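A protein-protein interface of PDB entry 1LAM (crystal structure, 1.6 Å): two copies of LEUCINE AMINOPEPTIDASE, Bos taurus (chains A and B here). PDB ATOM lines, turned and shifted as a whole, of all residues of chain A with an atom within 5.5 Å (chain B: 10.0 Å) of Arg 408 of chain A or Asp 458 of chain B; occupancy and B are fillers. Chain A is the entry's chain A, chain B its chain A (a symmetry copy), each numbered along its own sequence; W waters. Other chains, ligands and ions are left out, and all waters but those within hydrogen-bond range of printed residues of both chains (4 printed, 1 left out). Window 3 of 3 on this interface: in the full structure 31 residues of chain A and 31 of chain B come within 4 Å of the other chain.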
ATOM      1  N   GLU A 404       3.785  19.988 -18.239  1.00  0.00           N
ATOM      2  CA  GLU A 404       2.504  19.614 -17.629  1.00  0.00           C
ATOM      3  C   GLU A 404       1.419  19.582 -18.720  1.00  0.00           C
ATOM      4  O   GLU A 404       0.410  18.881 -18.592  1.00  0.00           O
ATOM      5  CB  GLU A 404       2.130  20.577 -16.492  1.00  0.00           C
ATOM      6  CG  GLU A 404       0.788  20.271 -15.785  1.00  0.00           C
ATOM      7  CD  GLU A 404      -0.426  20.864 -16.501  1.00  0.00           C
ATOM      8  OE1 GLU A 404      -0.260  21.788 -17.334  1.00  0.00           O
ATOM      9  OE2 GLU A 404      -1.557  20.407 -16.235  1.00  0.00           O
ATOM     10  N   HIS A 405       1.627  20.370 -19.770  1.00  0.00           N
ATOM     11  CA  HIS A 405       0.747  20.421 -20.941  1.00  0.00           C
ATOM     12  C   HIS A 405       0.413  18.978 -21.382  1.00  0.00           C
ATOM     13  O   HIS A 405      -0.740  18.653 -21.689  1.00  0.00           O
ATOM     14  CB  HIS A 405       1.504  21.157 -22.068  1.00  0.00           C
ATOM     15  CG  HIS A 405       0.802  21.171 -23.398  1.00  0.00           C
ATOM     16  ND1 HIS A 405       0.697  20.060 -24.213  1.00  0.00           N
ATOM     17  CD2 HIS A 405       0.221  22.191 -24.077  1.00  0.00           C
ATOM     18  CE1 HIS A 405       0.078  20.394 -25.333  1.00  0.00           C
ATOM     19  NE2 HIS A 405      -0.225  21.681 -25.272  1.00  0.00           N
ATOM     20  N   TYR A 406       1.429  18.120 -21.390  1.00  0.00           N
ATOM     21  CA  TYR A 406       1.257  16.732 -21.807  1.00  0.00           C
ATOM     22  C   TYR A 406       0.668  15.881 -20.685  1.00  0.00           C
ATOM     23  O   TYR A 406      -0.184  15.015 -20.930  1.00  0.00           O
ATOM     24  CB  TYR A 406       2.590  16.158 -22.305  1.00  0.00           C
ATOM     25  CG  TYR A 406       3.188  16.969 -23.438  1.00  0.00           C
ATOM     26  CD1 TYR A 406       2.519  17.090 -24.664  1.00  0.00           C
ATOM     27  CD2 TYR A 406       4.392  17.651 -23.274  1.00  0.00           C
ATOM     28  CE1 TYR A 406       3.038  17.874 -25.694  1.00  0.00           C
ATOM     29  CE2 TYR A 406       4.920  18.441 -24.293  1.00  0.00           C
ATOM     30  CZ  TYR A 406       4.242  18.551 -25.502  1.00  0.00           C
ATOM     31  OH  TYR A 406       4.759  19.338 -26.515  1.00  0.00           O
ATOM     32  N   THR A 407       1.058  16.175 -19.447  1.00  0.00           N
ATOM     33  CA  THR A 407       0.548  15.444 -18.283  1.00  0.00           C
ATOM     34  C   THR A 407      -0.976  15.556 -18.173  1.00  0.00           C
ATOM     35  O   THR A 407      -1.669  14.583 -17.867  1.00  0.00           O
ATOM     36  CB  THR A 407       1.148  15.997 -16.987  1.00  0.00           C
ATOM     37  OG1 THR A 407       2.578  15.946 -17.055  1.00  0.00           O
ATOM     38  CG2 THR A 407       0.642  15.210 -15.784  1.00  0.00           C
ATOM     39  N   ARG A 408      -1.481  16.754 -18.435  1.00  0.00           N
ATOM     40  CA  ARG A 408      -2.905  17.040 -18.358  1.00  0.00           C
ATOM     41  C   ARG A 408      -3.698  16.094 -19.262  1.00  0.00           C
ATOM     42  O   ARG A 408      -4.796  15.633 -18.916  1.00  0.00           O
ATOM     43  CB  ARG A 408      -3.141  18.504 -18.752  1.00  0.00           C
ATOM     44  CG  ARG A 408      -4.557  18.980 -18.618  1.00  0.00           C
ATOM     45  CD  ARG A 408      -4.690  20.421 -19.079  1.00  0.00           C
ATOM     46  NE  ARG A 408      -6.091  20.839 -19.088  1.00  0.00           N
ATOM     47  CZ  ARG A 408      -6.576  21.861 -19.789  1.00  0.00           C
ATOM     48  NH1 ARG A 408      -5.776  22.594 -20.563  1.00  0.00           N
ATOM     49  NH2 ARG A 408      -7.869  22.149 -19.715  1.00  0.00           N
ATOM     50  N   GLN A 409      -3.092  15.741 -20.385  1.00  0.00           N
ATOM     51  CA  GLN A 409      -3.744  14.868 -21.348  1.00  0.00           C
ATOM     52  C   GLN A 409      -3.794  13.386 -20.980  1.00  0.00           C
ATOM     53  O   GLN A 409      -4.516  12.614 -21.616  1.00  0.00           O
ATOM     54  CB  GLN A 409      -3.131  15.093 -22.728  1.00  0.00           C
ATOM     55  CG  GLN A 409      -3.364  16.533 -23.201  1.00  0.00           C
ATOM     56  CD  GLN A 409      -2.734  16.861 -24.533  1.00  0.00           C
ATOM     57  OE1 GLN A 409      -2.474  18.031 -24.836  1.00  0.00           O
ATOM     58  NE2 GLN A 409      -2.484  15.849 -25.340  1.00  0.00           N
ATOM     59  N   VAL A 410      -3.024  12.988 -19.967  1.00  0.00           N
ATOM     60  CA  VAL A 410      -3.041  11.604 -19.513  1.00  0.00           C
ATOM     61  C   VAL A 410      -3.699  11.438 -18.135  1.00  0.00           C
ATOM     62  O   VAL A 410      -4.081  10.335 -17.757  1.00  0.00           O
ATOM     63  CB  VAL A 410      -1.643  10.940 -19.551  1.00  0.00           C
ATOM     64  CG1 VAL A 410      -1.089  10.974 -20.972  1.00  0.00           C
ATOM     65  CG2 VAL A 410      -0.697  11.622 -18.578  1.00  0.00           C
ATOM     66  N   ILE A 411      -3.788  12.508 -17.347  1.00  0.00           N
ATOM     67  CA  ILE A 411      -4.467  12.369 -16.066  1.00  0.00           C
ATOM     68  C   ILE A 411      -5.951  12.716 -16.217  1.00  0.00           C
ATOM     69  O   ILE A 411      -6.733  12.524 -15.290  1.00  0.00           O
ATOM     70  CB  ILE A 411      -3.786  13.115 -14.906  1.00  0.00           C
ATOM     71  CG1 ILE A 411      -3.702  14.604 -15.185  1.00  0.00           C
ATOM     72  CG2 ILE A 411      -2.397  12.535 -14.647  1.00  0.00           C
ATOM     73  CD1 ILE A 411      -2.979  15.341 -14.055  1.00  0.00           C
ATOM     74  N   ASP A 412      -6.336  13.213 -17.390  1.00  0.00           N
ATOM     75  CA  ASP A 412      -7.742  13.486 -17.703  1.00  0.00           C
ATOM     76  C   ASP A 412      -8.166  12.042 -18.026  1.00  0.00           C
ATOM     77  O   ASP A 412      -7.995  11.574 -19.150  1.00  0.00           O
ATOM     78  CB  ASP A 412      -7.836  14.363 -18.957  1.00  0.00           C
ATOM     79  CG  ASP A 412      -9.279  14.640 -19.391  1.00  0.00           C
ATOM     80  OD1 ASP A 412     -10.070  13.686 -19.562  1.00  0.00           O
ATOM     81  OD2 ASP A 412      -9.613  15.824 -19.612  1.00  0.00           O
ATOM     82  N   LYS A 423      -5.389  11.909 -24.556  1.00  0.00           N
ATOM     83  CA  LYS A 423      -6.702  12.370 -25.020  1.00  0.00           C
ATOM     84  C   LYS A 423      -6.752  12.519 -26.542  1.00  0.00           C
ATOM     85  O   LYS A 423      -7.780  12.257 -27.164  1.00  0.00           O
ATOM     86  CB  LYS A 423      -7.014  13.739 -24.410  1.00  0.00           C
ATOM     87  CG  LYS A 423      -7.710  13.719 -23.082  1.00  0.00           C
ATOM     88  CD  LYS A 423      -7.295  14.948 -22.268  1.00  0.00           C
ATOM     89  CE  LYS A 423      -7.611  16.254 -22.959  1.00  0.00           C
ATOM     90  NZ  LYS A 423      -8.999  16.732 -22.670  1.00  0.00           N
ATOM     91  N   TYR A 424      -5.653  13.010 -27.112  1.00  0.00           N
ATOM     92  CA  TYR A 424      -5.534  13.253 -28.545  1.00  0.00           C
ATOM     93  C   TYR A 424      -4.424  12.395 -29.156  1.00  0.00           C
ATOM     94  O   TYR A 424      -3.667  11.729 -28.455  1.00  0.00           O
ATOM     95  CB  TYR A 424      -5.225  14.738 -28.802  1.00  0.00           C
ATOM     96  CG  TYR A 424      -6.026  15.732 -27.971  1.00  0.00           C
ATOM     97  CD1 TYR A 424      -7.419  15.799 -28.061  1.00  0.00           C
ATOM     98  CD2 TYR A 424      -5.382  16.633 -27.122  1.00  0.00           C
ATOM     99  CE1 TYR A 424      -8.147  16.742 -27.324  1.00  0.00           C
ATOM    100  CE2 TYR A 424      -6.091  17.580 -26.385  1.00  0.00           C
ATOM    101  CZ  TYR A 424      -7.474  17.633 -26.486  1.00  0.00           C
ATOM    102  OH  TYR A 424      -8.185  18.573 -25.750  1.00  0.00           O
ATOM    103  N   LYS B  50      -9.112  29.924 -11.287  1.00  0.00           N
ATOM    104  CA  LYS B  50     -10.509  29.772 -10.875  1.00  0.00           C
ATOM    105  C   LYS B  50     -11.115  31.148 -10.638  1.00  0.00           C
ATOM    106  O   LYS B  50     -10.386  32.109 -10.389  1.00  0.00           O
ATOM    107  CB  LYS B  50     -10.608  28.934  -9.600  1.00  0.00           C
ATOM    108  CG  LYS B  50     -10.149  27.512  -9.775  1.00  0.00           C
ATOM    109  CD  LYS B  50     -11.005  26.822 -10.831  1.00  0.00           C
ATOM    110  CE  LYS B  50     -10.648  25.350 -11.001  1.00  0.00           C
ATOM    111  NZ  LYS B  50     -11.623  24.701 -11.925  1.00  0.00           N
ATOM    112  N   GLU B  80       9.338  24.233 -17.073  1.00  0.00           N
ATOM    113  CA  GLU B  80       8.382  24.557 -18.122  1.00  0.00           C
ATOM    114  C   GLU B  80       8.886  25.551 -19.169  1.00  0.00           C
ATOM    115  O   GLU B  80       8.236  25.764 -20.201  1.00  0.00           O
ATOM    116  CB  GLU B  80       7.065  25.049 -17.506  1.00  0.00           C
ATOM    117  CG  GLU B  80       6.368  24.045 -16.580  1.00  0.00           C
ATOM    118  CD  GLU B  80       5.725  22.878 -17.323  1.00  0.00           C
ATOM    119  OE1 GLU B  80       5.566  22.949 -18.561  1.00  0.00           O
ATOM    120  OE2 GLU B  80       5.376  21.879 -16.666  1.00  0.00           O
ATOM    121  N   TRP B  82       9.067  28.846 -19.106  1.00  0.00           N
ATOM    122  CA  TRP B  82       8.249  30.045 -19.265  1.00  0.00           C
ATOM    123  C   TRP B  82       8.148  30.774 -17.936  1.00  0.00           C
ATOM    124  O   TRP B  82       8.560  30.244 -16.895  1.00  0.00           O
ATOM    125  CB  TRP B  82       6.845  29.757 -19.835  1.00  0.00           C
ATOM    126  CG  TRP B  82       5.909  28.896 -19.003  1.00  0.00           C
ATOM    127  CD1 TRP B  82       6.014  28.578 -17.677  1.00  0.00           C
ATOM    128  CD2 TRP B  82       4.732  28.232 -19.481  1.00  0.00           C
ATOM    129  NE1 TRP B  82       4.986  27.747 -17.296  1.00  0.00           N
ATOM    130  CE2 TRP B  82       4.181  27.513 -18.393  1.00  0.00           C
ATOM    131  CE3 TRP B  82       4.090  28.159 -20.730  1.00  0.00           C
ATOM    132  CZ2 TRP B  82       3.018  26.742 -18.506  1.00  0.00           C
ATOM    133  CZ3 TRP B  82       2.935  27.391 -20.852  1.00  0.00           C
ATOM    134  CH2 TRP B  82       2.414  26.690 -19.746  1.00  0.00           C
ATOM    135  N   GLU B  87       1.920  33.557 -17.023  1.00  0.00           N
ATOM    136  CA  GLU B  87       0.942  32.581 -17.517  1.00  0.00           C
ATOM    137  C   GLU B  87      -0.291  32.479 -16.606  1.00  0.00           C
ATOM    138  O   GLU B  87      -1.418  32.355 -17.098  1.00  0.00           O
ATOM    139  CB  GLU B  87       1.599  31.200 -17.723  1.00  0.00           C
ATOM    140  CG  GLU B  87       2.293  31.059 -19.069  1.00  0.00           C
ATOM    141  CD  GLU B  87       1.317  31.089 -20.229  1.00  0.00           C
ATOM    142  OE1 GLU B  87       0.437  30.208 -20.289  1.00  0.00           O
ATOM    143  OE2 GLU B  87       1.427  31.993 -21.085  1.00  0.00           O
ATOM    144  N   ALA B  91      -4.219  33.508 -17.868  1.00  0.00           N
ATOM    145  CA  ALA B  91      -5.289  32.531 -17.704  1.00  0.00           C
ATOM    146  C   ALA B  91      -6.393  33.031 -16.773  1.00  0.00           C
ATOM    147  O   ALA B  91      -7.573  32.934 -17.100  1.00  0.00           O
ATOM    148  CB  ALA B  91      -4.715  31.221 -17.190  1.00  0.00           C
ATOM    149  N   ARG B  98     -14.367  36.180 -19.411  1.00  0.00           N
ATOM    150  CA  ARG B  98     -15.400  35.330 -20.010  1.00  0.00           C
ATOM    151  C   ARG B  98     -16.663  35.261 -19.130  1.00  0.00           C
ATOM    152  O   ARG B  98     -17.781  35.135 -19.637  1.00  0.00           O
ATOM    153  CB  ARG B  98     -14.855  33.934 -20.305  1.00  0.00           C
ATOM    154  CG  ARG B  98     -13.803  33.917 -21.419  1.00  0.00           C
ATOM    155  CD  ARG B  98     -13.465  32.499 -21.838  1.00  0.00           C
ATOM    156  NE  ARG B  98     -13.213  31.638 -20.683  1.00  0.00           N
ATOM    157  CZ  ARG B  98     -12.004  31.283 -20.240  1.00  0.00           C
ATOM    158  NH1 ARG B  98     -10.908  31.678 -20.884  1.00  0.00           N
ATOM    159  NH2 ARG B  98     -11.904  30.497 -19.166  1.00  0.00           N
ATOM    160  N   SER B 370       0.611  20.644 -29.622  1.00  0.00           N
ATOM    161  CA  SER B 370       0.456  22.082 -29.424  1.00  0.00           C
ATOM    162  C   SER B 370       1.297  22.600 -28.256  1.00  0.00           C
ATOM    163  O   SER B 370       1.122  23.743 -27.818  1.00  0.00           O
ATOM    164  CB  SER B 370      -1.019  22.439 -29.209  1.00  0.00           C
ATOM    165  OG  SER B 370      -1.513  21.848 -28.026  1.00  0.00           O
ATOM    166  N   ARG B 396       5.679  29.009 -26.210  1.00  0.00           N
ATOM    167  CA  ARG B 396       6.908  28.233 -26.306  1.00  0.00           C
ATOM    168  C   ARG B 396       7.420  27.708 -27.638  1.00  0.00           C
ATOM    169  O   ARG B 396       6.648  27.432 -28.557  1.00  0.00           O
ATOM    170  CB  ARG B 396       6.857  27.104 -25.272  1.00  0.00           C
ATOM    171  CG  ARG B 396       6.564  27.593 -23.854  1.00  0.00           C
ATOM    172  CD  ARG B 396       6.552  26.454 -22.837  1.00  0.00           C
ATOM    173  NE  ARG B 396       5.318  25.653 -22.873  1.00  0.00           N
ATOM    174  CZ  ARG B 396       4.953  24.801 -21.917  1.00  0.00           C
ATOM    175  NH1 ARG B 396       5.741  24.612 -20.862  1.00  0.00           N
ATOM    176  NH2 ARG B 396       3.813  24.127 -22.023  1.00  0.00           N
ATOM    177  N   THR B 455      -4.080  25.253 -34.096  1.00  0.00           N
ATOM    178  CA  THR B 455      -5.349  25.403 -33.408  1.00  0.00           C
ATOM    179  C   THR B 455      -5.211  25.249 -31.901  1.00  0.00           C
ATOM    180  O   THR B 455      -4.188  24.772 -31.399  1.00  0.00           O
ATOM    181  CB  THR B 455      -6.346  24.310 -33.861  1.00  0.00           C
ATOM    182  OG1 THR B 455      -5.934  23.040 -33.333  1.00  0.00           O
ATOM    183  CG2 THR B 455      -6.386  24.201 -35.376  1.00  0.00           C
ATOM    184  N   ASN B 456      -6.285  25.608 -31.202  1.00  0.00           N
ATOM    185  CA  ASN B 456      -6.369  25.462 -29.760  1.00  0.00           C
ATOM    186  C   ASN B 456      -7.739  24.873 -29.437  1.00  0.00           C
ATOM    187  O   ASN B 456      -8.742  25.206 -30.075  1.00  0.00           O
ATOM    188  CB  ASN B 456      -6.234  26.802 -29.023  1.00  0.00           C
ATOM    189  CG  ASN B 456      -6.115  26.627 -27.501  1.00  0.00           C
ATOM    190  OD1 ASN B 456      -5.129  26.088 -26.998  1.00  0.00           O
ATOM    191  ND2 ASN B 456      -7.119  27.094 -26.767  1.00  0.00           N
ATOM    192  N   LYS B 457      -7.740  23.911 -28.523  1.00  0.00           N
ATOM    193  CA  LYS B 457      -8.958  23.299 -28.037  1.00  0.00           C
ATOM    194  C   LYS B 457      -9.115  23.944 -26.663  1.00  0.00           C
ATOM    195  O   LYS B 457      -9.869  24.892 -26.524  1.00  0.00           O
ATOM    196  CB  LYS B 457      -8.793  21.785 -27.935  1.00  0.00           C
ATOM    197  CG  LYS B 457      -8.509  21.138 -29.282  1.00  0.00           C
ATOM    198  CD  LYS B 457      -8.430  19.626 -29.157  1.00  0.00           C
ATOM    199  CE  LYS B 457      -7.808  18.997 -30.385  1.00  0.00           C
ATOM    200  NZ  LYS B 457      -6.354  19.295 -30.493  1.00  0.00           N
ATOM    201  N   ASP B 458      -8.278  23.519 -25.714  1.00  0.00           N
ATOM    202  CA  ASP B 458      -8.273  24.053 -24.344  1.00  0.00           C
ATOM    203  C   ASP B 458      -6.877  24.067 -23.720  1.00  0.00           C
ATOM    204  O   ASP B 458      -6.728  24.376 -22.541  1.00  0.00           O
ATOM    205  CB  ASP B 458      -9.194  23.215 -23.436  1.00  0.00           C
ATOM    206  CG  ASP B 458      -8.677  21.779 -23.214  1.00  0.00           C
ATOM    207  OD1 ASP B 458      -7.770  21.281 -23.938  1.00  0.00           O
ATOM    208  OD2 ASP B 458      -9.214  21.129 -22.300  1.00  0.00           O
ATOM    209  N   GLU B 459      -5.860  23.751 -24.515  1.00  0.00           N
ATOM    210  CA  GLU B 459      -4.483  23.678 -24.010  1.00  0.00           C
ATOM    211  C   GLU B 459      -3.993  25.016 -23.459  1.00  0.00           C
ATOM    212  O   GLU B 459      -3.416  25.049 -22.372  1.00  0.00           O
ATOM    213  CB  GLU B 459      -3.526  23.164 -25.089  1.00  0.00           C
ATOM    214  CG  GLU B 459      -3.933  21.817 -25.691  1.00  0.00           C
ATOM    215  CD  GLU B 459      -4.681  21.981 -27.000  1.00  0.00           C
ATOM    216  OE1 GLU B 459      -5.717  22.677 -27.027  1.00  0.00           O
ATOM    217  OE2 GLU B 459      -4.223  21.421 -28.017  1.00  0.00           O
ATOM    218  N   VAL B 460      -4.139  26.087 -24.239  1.00  0.00           N
ATOM    219  CA  VAL B 460      -3.766  27.433 -23.792  1.00  0.00           C
ATOM    220  C   VAL B 460      -5.085  27.947 -23.205  1.00  0.00           C
ATOM    221  O   VAL B 460      -6.041  28.217 -23.932  1.00  0.00           O
ATOM    222  CB  VAL B 460      -3.299  28.308 -24.986  1.00  0.00           C
ATOM    223  CG1 VAL B 460      -2.903  29.696 -24.497  1.00  0.00           C
ATOM    224  CG2 VAL B 460      -2.118  27.645 -25.690  1.00  0.00           C
ATOM    225  N   PRO B 461      -5.153  28.098 -21.872  1.00  0.00           N
ATOM    226  CA  PRO B 461      -6.358  28.555 -21.169  1.00  0.00           C
ATOM    227  C   PRO B 461      -6.983  29.849 -21.648  1.00  0.00           C
ATOM    228  O   PRO B 461      -8.197  30.003 -21.628  1.00  0.00           O
ATOM    229  CB  PRO B 461      -5.876  28.705 -19.724  1.00  0.00           C
ATOM    230  CG  PRO B 461      -4.676  27.808 -19.637  1.00  0.00           C
ATOM    231  CD  PRO B 461      -4.008  28.063 -20.951  1.00  0.00           C
ATOM    232  N   TYR B 462      -6.143  30.782 -22.069  1.00  0.00           N
ATOM    233  CA  TYR B 462      -6.617  32.077 -22.515  1.00  0.00           C
ATOM    234  C   TYR B 462      -6.971  32.201 -23.995  1.00  0.00           C
ATOM    235  O   TYR B 462      -7.109  33.307 -24.503  1.00  0.00           O
ATOM    236  CB  TYR B 462      -5.643  33.173 -22.081  1.00  0.00           C
ATOM    237  CG  TYR B 462      -4.183  32.886 -22.401  1.00  0.00           C
ATOM    238  CD1 TYR B 462      -3.617  33.302 -23.614  1.00  0.00           C
ATOM    239  CD2 TYR B 462      -3.350  32.253 -21.467  1.00  0.00           C
ATOM    240  CE1 TYR B 462      -2.257  33.101 -23.886  1.00  0.00           C
ATOM    241  CE2 TYR B 462      -1.988  32.053 -21.725  1.00  0.00           C
ATOM    242  CZ  TYR B 462      -1.451  32.478 -22.936  1.00  0.00           C
ATOM    243  OH  TYR B 462      -0.120  32.292 -23.207  1.00  0.00           O
ATOM    244  N   LEU B 463      -7.087  31.079 -24.701  1.00  0.00           N
ATOM    245  CA  LEU B 463      -7.480  31.122 -26.115  1.00  0.00           C
ATOM    246  C   LEU B 463      -8.724  30.262 -26.263  1.00  0.00           C
ATOM    247  O   LEU B 463      -8.715  29.103 -25.861  1.00  0.00           O
ATOM    248  CB  LEU B 463      -6.382  30.558 -27.033  1.00  0.00           C
ATOM    249  CG  LEU B 463      -5.048  31.302 -27.107  1.00  0.00           C
ATOM    250  CD1 LEU B 463      -4.064  30.490 -27.939  1.00  0.00           C
ATOM    251  CD2 LEU B 463      -5.243  32.699 -27.689  1.00  0.00           C
ATOM    252  N   ARG B 464      -9.804  30.817 -26.794  1.00  0.00           N
ATOM    253  CA  ARG B 464     -11.009  30.016 -27.000  1.00  0.00           C
ATOM    254  C   ARG B 464     -10.723  29.017 -28.134  1.00  0.00           C
ATOM    255  O   ARG B 464      -9.719  29.145 -28.844  1.00  0.00           O
ATOM    256  CB  ARG B 464     -12.196  30.921 -27.348  1.00  0.00           C
ATOM    257  CG  ARG B 464     -12.797  31.609 -26.123  1.00  0.00           C
ATOM    258  CD  ARG B 464     -13.836  32.680 -26.479  1.00  0.00           C
ATOM    259  NE  ARG B 464     -14.775  32.853 -25.377  1.00  0.00           N
ATOM    260  CZ  ARG B 464     -15.348  34.005 -25.037  1.00  0.00           C
ATOM    261  NH1 ARG B 464     -15.093  35.120 -25.714  1.00  0.00           N
ATOM    262  NH2 ARG B 464     -16.197  34.036 -24.014  1.00  0.00           N
ATOM    263  N   LYS B 465     -11.580  28.014 -28.296  1.00  0.00           N
ATOM    264  CA  LYS B 465     -11.396  26.998 -29.333  1.00  0.00           C
ATOM    265  C   LYS B 465     -11.358  27.592 -30.752  1.00  0.00           C
ATOM    266  O   LYS B 465     -12.239  28.367 -31.136  1.00  0.00           O
ATOM    267  CB  LYS B 465     -12.517  25.970 -29.208  1.00  0.00           C
ATOM    268  CG  LYS B 465     -12.335  24.698 -30.032  1.00  0.00           C
ATOM    269  CD  LYS B 465     -13.494  23.725 -29.785  1.00  0.00           C
ATOM    270  CE  LYS B 465     -13.780  23.501 -28.272  1.00  0.00           C
ATOM    271  NZ  LYS B 465     -12.716  22.754 -27.468  1.00  0.00           N
ATOM    272  N   GLY B 466     -10.338  27.226 -31.523  1.00  0.00           N
ATOM    273  CA  GLY B 466     -10.204  27.736 -32.879  1.00  0.00           C
ATOM    274  C   GLY B 466      -8.755  27.999 -33.270  1.00  0.00           C
ATOM    275  O   GLY B 466      -7.832  27.582 -32.561  1.00  0.00           O
ATOM    276  N   ALA B 468      -5.232  29.428 -33.522  1.00  0.00           N
ATOM    277  CA  ALA B 468      -4.483  30.064 -32.449  1.00  0.00           C
ATOM    278  C   ALA B 468      -3.631  31.307 -32.712  1.00  0.00           C
ATOM    279  O   ALA B 468      -3.396  32.086 -31.782  1.00  0.00           O
ATOM    280  CB  ALA B 468      -3.653  29.004 -31.721  1.00  0.00           C
ATOM    281  N   ARG B 470      -0.510  31.395 -33.170  1.00  0.00           N
ATOM    282  CA  ARG B 470       0.763  31.180 -32.467  1.00  0.00           C
ATOM    283  C   ARG B 470       1.836  30.930 -33.519  1.00  0.00           C
ATOM    284  O   ARG B 470       1.560  30.292 -34.543  1.00  0.00           O
ATOM    285  CB  ARG B 470       0.663  29.948 -31.551  1.00  0.00           C
ATOM    286  CG  ARG B 470      -0.413  30.044 -30.452  1.00  0.00           C
ATOM    287  CD  ARG B 470      -0.622  28.748 -29.672  1.00  0.00           C
ATOM    288  NE  ARG B 470       0.615  28.282 -29.039  1.00  0.00           N
ATOM    289  CZ  ARG B 470       0.807  27.075 -28.509  1.00  0.00           C
ATOM    290  NH1 ARG B 470      -0.179  26.178 -28.495  1.00  0.00           N
ATOM    291  NH2 ARG B 470       1.991  26.766 -27.986  1.00  0.00           N
HETATM  292  O   HOH W   1      -7.745  25.333 -20.071  1.00  0.00           O
HETATM  293  O   HOH W   2      -3.304  18.856 -28.004  1.00  0.00           O
HETATM  294  O   HOH W   3      -2.927  22.833 -21.031  1.00  0.00           O
HETATM  295  O   HOH W   4      -0.602  18.848 -27.637  1.00  0.00           O
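No position is printed for both chains.
No residue of chain B comes within 4 Å of Thr 407 of chain A.
No residue of chain B comes within 4 Å of Ile 411 of chain A.
No residue of chain B comes within 4 Å of Asp 412 of chain A.
Of the printed residues of chain A, Glu 80 of chain B touches Glu 404.
Printed residues of chain A within 4 Å of Ser 370 of chain B: His 405.
Printed residues of chain A within 4 Å of Arg 396 of chain B: His 405 (3.8 Å).
Asp 458 of chain B touches just these residues of chain A: Arg 408 (2.8 Å) and Tyr 424 (3.3 Å).
Arg 464 of chain B touches none of the printed residues of chain A.
The nearest residue of chain B that does not touch Arg 408 of chain A is Val 460 of chain B (5.3 Å).
The nearest residue of chain A that does not touch Asp 458 of chain B is Lys 423 of chain A (4.4 Å).
Among the printed residues, merely in contact across the chains: Tyr 424 of chain A with Lys 457 of chain B (3.4 Å), His 405 of chain A with Glu 459 of chain B (3.6 Å), His 405 of chain A with Arg 396 of chain B (3.8 Å) and Arg 408 of chain A with Glu 459 of chain B (3.8 Å).
The side-chain carboxylate (OE1) of Glu 80 of chain B lies within salt-bridge range of the guanidinium group (NH1) of Arg 396 of chain B (2.8 Å).
The side-chain carboxylate (OE2) of Glu 459 of chain B sits at hydrogen-bond distance from the side-chain hydroxyl (OG) of Ser 370 of chain B (2.7 Å).
O of Ser 370 of chain B sits at hydrogen-bond distance from NH1 of Arg 470 of chain B, at 2.8 Å.
The side-chain carboxylate of Glu 459 of chain B sits close to the side-chain amide oxygen of Asn 456 of chain B (3.5 Å).
NZ of Lys 457 of chain B is in salt-bridge range of OE2 of Glu 459 of chain B (3.9 Å).
The backbone NH (N) of Glu 404 of chain A is in hydrogen-bond range of the side-chain carboxylate (OE2) of Glu 80 of chain B (2.9 Å).
OG of Ser 370 of chain B lies within hydrogen-bond range of NE2 of His 405 of chain A, 3.0 Å away.
NH2 of Arg 408 of chain A lies within salt-bridge range of OD2 of Asp 458 of chain B (3.1 Å).
The side-chain carboxylate (OD1) of Asp 458 of chain B sits at hydrogen-bond distance from the side-chain hydroxyl (OH) of Tyr 424 of chain A.
Printed residues of chain B that touch a printed residue of chain A: Glu 80, Ser 370, Arg 396, Lys 457, Asp 458 and Glu 459.
Among the printed residues, Asp or Glu carboxylates within 4 Å of a Lys or Arg side-chain nitrogen of the other chain: Arg 408 of chain A with Asp 458 of chain B (3.1 Å).
Water W3 bridges O of Glu 459 of chain B and NH1 of Arg 408 of chain A.
Water W2 lies within hydrogen-bond range of the side-chain carboxylate (OE2) of Glu 459 of chain B (2.7 Å), the side-chain amide oxygen (OE1) of Gln 409 of chain A (3.4 Å) and the side-chain hydroxyl (OG) of Ser 370 of chain B (3.5 Å).
Water W1 bridges O of Asp 458 of chain B and NH2 of Arg 408 of chain A.
Water W4 bridges the backbone NH of Ser 370 of chain B (2.9 Å) and the side-chain amide oxygen of Gln 409 of chain A (3.5 Å).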
